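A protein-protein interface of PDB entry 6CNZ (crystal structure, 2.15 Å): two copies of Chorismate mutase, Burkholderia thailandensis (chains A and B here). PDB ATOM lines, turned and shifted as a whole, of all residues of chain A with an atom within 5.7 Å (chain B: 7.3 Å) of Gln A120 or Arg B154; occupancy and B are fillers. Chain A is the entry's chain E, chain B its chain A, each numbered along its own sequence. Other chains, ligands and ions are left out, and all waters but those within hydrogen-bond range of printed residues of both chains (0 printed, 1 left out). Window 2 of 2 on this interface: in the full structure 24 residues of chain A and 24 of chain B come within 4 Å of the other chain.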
ATOM      1  N   ARG A  61       6.615   3.285   0.747  1.00  0.00           N
ATOM      2  CA  ARG A  61       7.719   3.705  -0.109  1.00  0.00           C
ATOM      3  C   ARG A  61       7.292   4.828  -1.041  1.00  0.00           C
ATOM      4  O   ARG A  61       8.075   5.743  -1.314  1.00  0.00           O
ATOM      5  CB  ARG A  61       8.253   2.526  -0.915  1.00  0.00           C
ATOM      6  CG  ARG A  61       8.827   1.396  -0.089  1.00  0.00           C
ATOM      7  CD  ARG A  61       9.059   0.194  -0.989  1.00  0.00           C
ATOM      8  NE  ARG A  61       9.707  -0.919  -0.314  1.00  0.00           N
ATOM      9  CZ  ARG A  61      10.990  -1.223  -0.454  1.00  0.00           C
ATOM     10  NH1 ARG A  61      11.765  -0.490  -1.244  1.00  0.00           N
ATOM     11  NH2 ARG A  61      11.501  -2.261   0.194  1.00  0.00           N
ATOM     12  N   ASP A 116      10.921  -8.847  -4.306  1.00  0.00           N
ATOM     13  CA  ASP A 116      11.056  -7.729  -3.371  1.00  0.00           C
ATOM     14  C   ASP A 116      11.981  -6.647  -3.912  1.00  0.00           C
ATOM     15  O   ASP A 116      11.724  -5.454  -3.721  1.00  0.00           O
ATOM     16  CB  ASP A 116      11.582  -8.219  -2.022  1.00  0.00           C
ATOM     17  CG  ASP A 116      10.652  -9.212  -1.358  1.00  0.00           C
ATOM     18  OD1 ASP A 116       9.434  -9.175  -1.636  1.00  0.00           O
ATOM     19  OD2 ASP A 116      11.142 -10.028  -0.551  1.00  0.00           O
ATOM     20  N   ARG A 117      13.084  -7.046  -4.556  1.00  0.00           N
ATOM     21  CA  ARG A 117      13.980  -6.061  -5.156  1.00  0.00           C
ATOM     22  C   ARG A 117      13.254  -5.230  -6.197  1.00  0.00           C
ATOM     23  O   ARG A 117      13.493  -4.028  -6.304  1.00  0.00           O
ATOM     24  CB  ARG A 117      15.184  -6.739  -5.799  1.00  0.00           C
ATOM     25  CG  ARG A 117      16.080  -7.489  -4.845  1.00  0.00           C
ATOM     26  CD  ARG A 117      17.417  -7.807  -5.504  1.00  0.00           C
ATOM     27  NE  ARG A 117      18.310  -6.654  -5.435  1.00  0.00           N
ATOM     28  CZ  ARG A 117      18.438  -5.740  -6.392  1.00  0.00           C
ATOM     29  NH1 ARG A 117      19.271  -4.724  -6.217  1.00  0.00           N
ATOM     30  NH2 ARG A 117      17.740  -5.845  -7.520  1.00  0.00           N
ATOM     31  N   LEU A 118      12.365  -5.854  -6.977  1.00  0.00           N
ATOM     32  CA  LEU A 118      11.659  -5.132  -8.031  1.00  0.00           C
ATOM     33  C   LEU A 118      10.630  -4.137  -7.500  1.00  0.00           C
ATOM     34  O   LEU A 118      10.317  -3.168  -8.195  1.00  0.00           O
ATOM     35  CB  LEU A 118      10.994  -6.123  -8.991  1.00  0.00           C
ATOM     36  CG  LEU A 118      12.035  -6.886  -9.817  1.00  0.00           C
ATOM     37  CD1 LEU A 118      11.433  -8.053 -10.571  1.00  0.00           C
ATOM     38  CD2 LEU A 118      12.766  -5.948 -10.773  1.00  0.00           C
ATOM     39  N   THR A 119      10.091  -4.343  -6.301  1.00  0.00           N
ATOM     40  CA  THR A 119       9.192  -3.344  -5.736  1.00  0.00           C
ATOM     41  C   THR A 119       9.892  -1.995  -5.623  1.00  0.00           C
ATOM     42  O   THR A 119       9.360  -0.967  -6.057  1.00  0.00           O
ATOM     43  CB  THR A 119       8.676  -3.800  -4.365  1.00  0.00           C
ATOM     44  OG1 THR A 119       7.837  -4.945  -4.522  1.00  0.00           O
ATOM     45  CG2 THR A 119       7.870  -2.708  -3.703  1.00  0.00           C
ATOM     46  N   GLN A 120      11.088  -1.979  -5.023  1.00  0.00           N
ATOM     47  CA  GLN A 120      11.867  -0.742  -4.943  1.00  0.00           C
ATOM     48  C   GLN A 120      12.157  -0.187  -6.337  1.00  0.00           C
ATOM     49  O   GLN A 120      11.917   0.997  -6.611  1.00  0.00           O
ATOM     50  CB  GLN A 120      13.168  -1.002  -4.172  1.00  0.00           C
ATOM     51  CG  GLN A 120      14.074   0.208  -3.980  1.00  0.00           C
ATOM     52  CD  GLN A 120      15.148   0.342  -5.066  1.00  0.00           C
ATOM     53  OE1 GLN A 120      15.381   1.440  -5.573  1.00  0.00           O
ATOM     54  NE2 GLN A 120      15.814  -0.773  -5.414  1.00  0.00           N
ATOM     55  N   SER A 121      12.653  -1.043  -7.241  1.00  0.00           N
ATOM     56  CA  SER A 121      13.009  -0.605  -8.588  1.00  0.00           C
ATOM     57  C   SER A 121      11.822   0.021  -9.310  1.00  0.00           C
ATOM     58  O   SER A 121      11.962   1.045  -9.994  1.00  0.00           O
ATOM     59  CB  SER A 121      13.550  -1.784  -9.395  1.00  0.00           C
ATOM     60  OG  SER A 121      14.739  -2.296  -8.821  1.00  0.00           O
ATOM     61  N   LEU A 122      10.650  -0.584  -9.173  1.00  0.00           N
ATOM     62  CA  LEU A 122       9.469  -0.094  -9.869  1.00  0.00           C
ATOM     63  C   LEU A 122       8.965   1.205  -9.263  1.00  0.00           C
ATOM     64  O   LEU A 122       8.463   2.077  -9.983  1.00  0.00           O
ATOM     65  CB  LEU A 122       8.378  -1.149  -9.820  1.00  0.00           C
ATOM     66  CG  LEU A 122       8.529  -2.258 -10.843  1.00  0.00           C
ATOM     67  CD1 LEU A 122       7.561  -3.369 -10.490  1.00  0.00           C
ATOM     68  CD2 LEU A 122       8.270  -1.702 -12.250  1.00  0.00           C
ATOM     69  N   ILE A 123       9.039   1.328  -7.936  1.00  0.00           N
ATOM     70  CA  ILE A 123       8.687   2.586  -7.293  1.00  0.00           C
ATOM     71  C   ILE A 123       9.528   3.716  -7.864  1.00  0.00           C
ATOM     72  O   ILE A 123       9.004   4.772  -8.248  1.00  0.00           O
ATOM     73  CB  ILE A 123       8.854   2.474  -5.769  1.00  0.00           C
ATOM     74  CG1 ILE A 123       7.741   1.604  -5.184  1.00  0.00           C
ATOM     75  CG2 ILE A 123       8.893   3.861  -5.132  1.00  0.00           C
ATOM     76  CD1 ILE A 123       6.364   2.150  -5.410  1.00  0.00           C
ATOM     77  N   ALA A 124      10.847   3.501  -7.943  1.00  0.00           N
ATOM     78  CA  ALA A 124      11.736   4.536  -8.462  1.00  0.00           C
ATOM     79  C   ALA A 124      11.467   4.804  -9.934  1.00  0.00           C
ATOM     80  O   ALA A 124      11.483   5.962 -10.366  1.00  0.00           O
ATOM     81  CB  ALA A 124      13.194   4.146  -8.249  1.00  0.00           C
ATOM     82  N   ALA A 125      11.198   3.753 -10.718  1.00  0.00           N
ATOM     83  CA  ALA A 125      10.879   3.963 -12.128  1.00  0.00           C
ATOM     84  C   ALA A 125       9.595   4.750 -12.270  1.00  0.00           C
ATOM     85  O   ALA A 125       9.486   5.641 -13.125  1.00  0.00           O
ATOM     86  CB  ALA A 125      10.752   2.627 -12.862  1.00  0.00           C
ATOM     87  N   TRP B 149      20.059   3.464 -15.030  1.00  0.00           N
ATOM     88  CA  TRP B 149      19.616   2.128 -14.657  1.00  0.00           C
ATOM     89  C   TRP B 149      20.168   1.732 -13.300  1.00  0.00           C
ATOM     90  O   TRP B 149      19.452   1.145 -12.484  1.00  0.00           O
ATOM     91  CB  TRP B 149      20.048   1.126 -15.729  1.00  0.00           C
ATOM     92  CG  TRP B 149      19.708  -0.271 -15.408  1.00  0.00           C
ATOM     93  CD1 TRP B 149      20.532  -1.202 -14.847  1.00  0.00           C
ATOM     94  CD2 TRP B 149      18.451  -0.924 -15.627  1.00  0.00           C
ATOM     95  NE1 TRP B 149      19.870  -2.388 -14.707  1.00  0.00           N
ATOM     96  CE2 TRP B 149      18.594  -2.253 -15.187  1.00  0.00           C
ATOM     97  CE3 TRP B 149      17.222  -0.516 -16.157  1.00  0.00           C
ATOM     98  CZ2 TRP B 149      17.550  -3.184 -15.254  1.00  0.00           C
ATOM     99  CZ3 TRP B 149      16.182  -1.444 -16.232  1.00  0.00           C
ATOM    100  CH2 TRP B 149      16.358  -2.764 -15.786  1.00  0.00           C
ATOM    101  N   LYS B 150      21.438   2.054 -13.031  1.00  0.00           N
ATOM    102  CA  LYS B 150      22.014   1.665 -11.751  1.00  0.00           C
ATOM    103  C   LYS B 150      21.279   2.329 -10.608  1.00  0.00           C
ATOM    104  O   LYS B 150      21.115   1.730  -9.532  1.00  0.00           O
ATOM    105  CB  LYS B 150      23.502   2.016 -11.694  1.00  0.00           C
ATOM    106  CG  LYS B 150      24.413   1.037 -12.444  1.00  0.00           C
ATOM    107  CD  LYS B 150      25.843   1.615 -12.458  1.00  0.00           C
ATOM    108  CE  LYS B 150      26.874   0.661 -13.044  1.00  0.00           C
ATOM    109  NZ  LYS B 150      28.183   1.378 -13.218  1.00  0.00           N
ATOM    110  N   THR B 151      20.807   3.554 -10.820  1.00  0.00           N
ATOM    111  CA  THR B 151      20.115   4.226  -9.729  1.00  0.00           C
ATOM    112  C   THR B 151      18.729   3.645  -9.497  1.00  0.00           C
ATOM    113  O   THR B 151      18.196   3.805  -8.403  1.00  0.00           O
ATOM    114  CB  THR B 151      20.023   5.729  -9.992  1.00  0.00           C
ATOM    115  OG1 THR B 151      19.257   5.954 -11.181  1.00  0.00           O
ATOM    116  CG2 THR B 151      21.420   6.323 -10.172  1.00  0.00           C
ATOM    117  N   LEU B 152      18.149   2.967 -10.498  1.00  0.00           N
ATOM    118  CA  LEU B 152      16.860   2.291 -10.338  1.00  0.00           C
ATOM    119  C   LEU B 152      17.007   0.971  -9.600  1.00  0.00           C
ATOM    120  O   LEU B 152      16.286   0.702  -8.635  1.00  0.00           O
ATOM    121  CB  LEU B 152      16.231   2.006 -11.705  1.00  0.00           C
ATOM    122  CG  LEU B 152      15.639   3.148 -12.499  1.00  0.00           C
ATOM    123  CD1 LEU B 152      15.100   2.622 -13.800  1.00  0.00           C
ATOM    124  CD2 LEU B 152      14.541   3.829 -11.671  1.00  0.00           C
ATOM    125  N   THR B 153      17.918   0.122 -10.073  1.00  0.00           N
ATOM    126  CA  THR B 153      17.988  -1.266  -9.649  1.00  0.00           C
ATOM    127  C   THR B 153      18.847  -1.467  -8.399  1.00  0.00           C
ATOM    128  O   THR B 153      18.504  -2.300  -7.559  1.00  0.00           O
ATOM    129  CB  THR B 153      18.502  -2.116 -10.814  1.00  0.00           C
ATOM    130  OG1 THR B 153      19.694  -1.530 -11.347  1.00  0.00           O
ATOM    131  CG2 THR B 153      17.450  -2.170 -11.909  1.00  0.00           C
ATOM    132  N   ARG B 154      19.952  -0.728  -8.243  1.00  0.00           N
ATOM    133  CA  ARG B 154      20.739  -0.744  -6.998  1.00  0.00           C
ATOM    134  C   ARG B 154      21.281  -2.145  -6.650  1.00  0.00           C
ATOM    135  O   ARG B 154      21.164  -2.626  -5.515  1.00  0.00           O
ATOM    136  CB  ARG B 154      19.914  -0.172  -5.834  1.00  0.00           C
ATOM    137  CG  ARG B 154      19.278   1.157  -6.172  1.00  0.00           C
ATOM    138  CD  ARG B 154      18.650   1.811  -4.953  1.00  0.00           C
ATOM    139  NE  ARG B 154      19.641   2.485  -4.118  1.00  0.00           N
ATOM    140  CZ  ARG B 154      20.005   3.761  -4.253  1.00  0.00           C
ATOM    141  NH1 ARG B 154      20.919   4.264  -3.437  1.00  0.00           N
ATOM    142  NH2 ARG B 154      19.466   4.535  -5.199  1.00  0.00           N
ATOM    143  N   TYR B 155      21.893  -2.804  -7.633  1.00  0.00           N
ATOM    144  CA  TYR B 155      22.618  -4.027  -7.348  1.00  0.00           C
ATOM    145  C   TYR B 155      23.911  -3.721  -6.582  1.00  0.00           C
ATOM    146  O   TYR B 155      24.384  -2.575  -6.519  1.00  0.00           O
ATOM    147  CB  TYR B 155      22.946  -4.773  -8.640  1.00  0.00           C
ATOM    148  CG  TYR B 155      21.767  -5.458  -9.298  1.00  0.00           C
ATOM    149  CD1 TYR B 155      21.292  -6.674  -8.817  1.00  0.00           C
ATOM    150  CD2 TYR B 155      21.141  -4.900 -10.415  1.00  0.00           C
ATOM    151  CE1 TYR B 155      20.233  -7.321  -9.432  1.00  0.00           C
ATOM    152  CE2 TYR B 155      20.080  -5.533 -11.032  1.00  0.00           C
ATOM    153  CZ  TYR B 155      19.628  -6.747 -10.535  1.00  0.00           C
ATOM    154  OH  TYR B 155      18.577  -7.393 -11.142  1.00  0.00           O
ATOM    155  N   ASP B 156      24.502  -4.782  -6.021  1.00  0.00           N
ATOM    156  CA  ASP B 156      25.770  -4.667  -5.304  1.00  0.00           C
ATOM    157  C   ASP B 156      26.893  -4.223  -6.252  1.00  0.00           C
ATOM    158  O   ASP B 156      26.787  -4.331  -7.477  1.00  0.00           O
ATOM    159  CB  ASP B 156      26.118  -5.998  -4.639  1.00  0.00           C
ATOM    160  CG  ASP B 156      26.282  -7.117  -5.638  1.00  0.00           C
ATOM    161  OD1 ASP B 156      27.326  -7.127  -6.316  1.00  0.00           O
ATOM    162  OD2 ASP B 156      25.374  -7.977  -5.754  1.00  0.00           O
ATOM    163  N   SER B 157      27.985  -3.719  -5.668  1.00  0.00           N
ATOM    164  CA  SER B 157      29.027  -3.101  -6.490  1.00  0.00           C
ATOM    165  C   SER B 157      29.680  -4.106  -7.436  1.00  0.00           C
ATOM    166  O   SER B 157      30.059  -3.754  -8.554  1.00  0.00           O
ATOM    167  CB  SER B 157      30.078  -2.439  -5.604  1.00  0.00           C
ATOM    168  OG  SER B 157      30.284  -3.203  -4.437  1.00  0.00           O
ATOM    169  N   LYS B 160      27.307  -4.233 -10.357  1.00  0.00           N
ATOM    170  CA  LYS B 160      27.377  -2.956 -11.052  1.00  0.00           C
ATOM    171  C   LYS B 160      28.697  -2.798 -11.800  1.00  0.00           C
ATOM    172  O   LYS B 160      28.716  -2.281 -12.922  1.00  0.00           O
ATOM    173  CB  LYS B 160      27.174  -1.817 -10.056  1.00  0.00           C
ATOM    174  CG  LYS B 160      25.738  -1.712  -9.554  1.00  0.00           C
ATOM    175  CD  LYS B 160      25.543  -0.390  -8.817  1.00  0.00           C
ATOM    176  CE  LYS B 160      26.553  -0.257  -7.704  1.00  0.00           C
ATOM    177  NZ  LYS B 160      26.217   0.869  -6.810  1.00  0.00           N
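Thr A119 touches none of the printed residues of chain B. Of the printed residues of chain B, Gln A120 touches Leu B152 (3.3 Å), Thr B153 (3.8 Å) and Arg B154 (3.3 Å). Of the printed residues of chain B, Ala A124 touches Leu B152. Of the printed residues of chain B, Ala A125 touches Leu B152. The nearest residue of chain B that does not touch Gln A120 is Thr B151 (4.6 Å).
Among the printed residues, pairs that only touch across the chains: Arg A117 with Tyr B155 (3.5 Å), Gln A120 with Thr B153 (3.8 Å), Gln A120 with Arg B154 (3.3 Å), Ser A121 with Thr B153 (3.5 Å), Ala A124 with Leu B152 (3.7 Å) and Ala A125 with Leu B152 (3.5 Å).
Printed residues of chain A that touch a printed residue of chain B: Arg A117, Gln A120, Ser A121, Ala A124 and Ala A125. Hydrophobic or aromatic side chains of chain A that line the printed part of chain B: Ala A124. Along chain A the printed residues that touch a printed residue of chain B span positions 117 to 125. Of the 10 printed residues of chain B, 4 touch a printed residue of chain A. Printed residues of chain B that touch a printed residue of chain A: Leu B152, Thr B153, Arg B154 and Tyr B155. Among the printed residues, 10 pairs touch across the chains. Among the printed residues, no Asp or Glu carboxylate lies within 4 Å of a Lys or Arg side-chain nitrogen of the other chain.
O of Arg A117 is in hydrogen-bond range of OG of Ser A121 (3.3 Å). O of Trp B149 lies within hydrogen-bond range of OG1 of Thr B153.
The backbone carbonyl oxygen (O) of Arg B154 sits at hydrogen-bond distance from the guanidinium group (NH1) of Arg A117 (2.9 Å). O of Leu B152 lies close to OE1 of Gln A120 (3.3 Å). OG of Ser A121 lies within hydrogen-bond range of O of Leu B152 (3.4 Å). The backbone carbonyl oxygen of Thr B153 sits at hydrogen-bond distance from the guanidinium group of Arg A117 (2.9 Å).
No position is printed for both chains. Of the 10 pairs that touch across the chains among the printed residues, none has its exchanged pair printed and touching as well.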
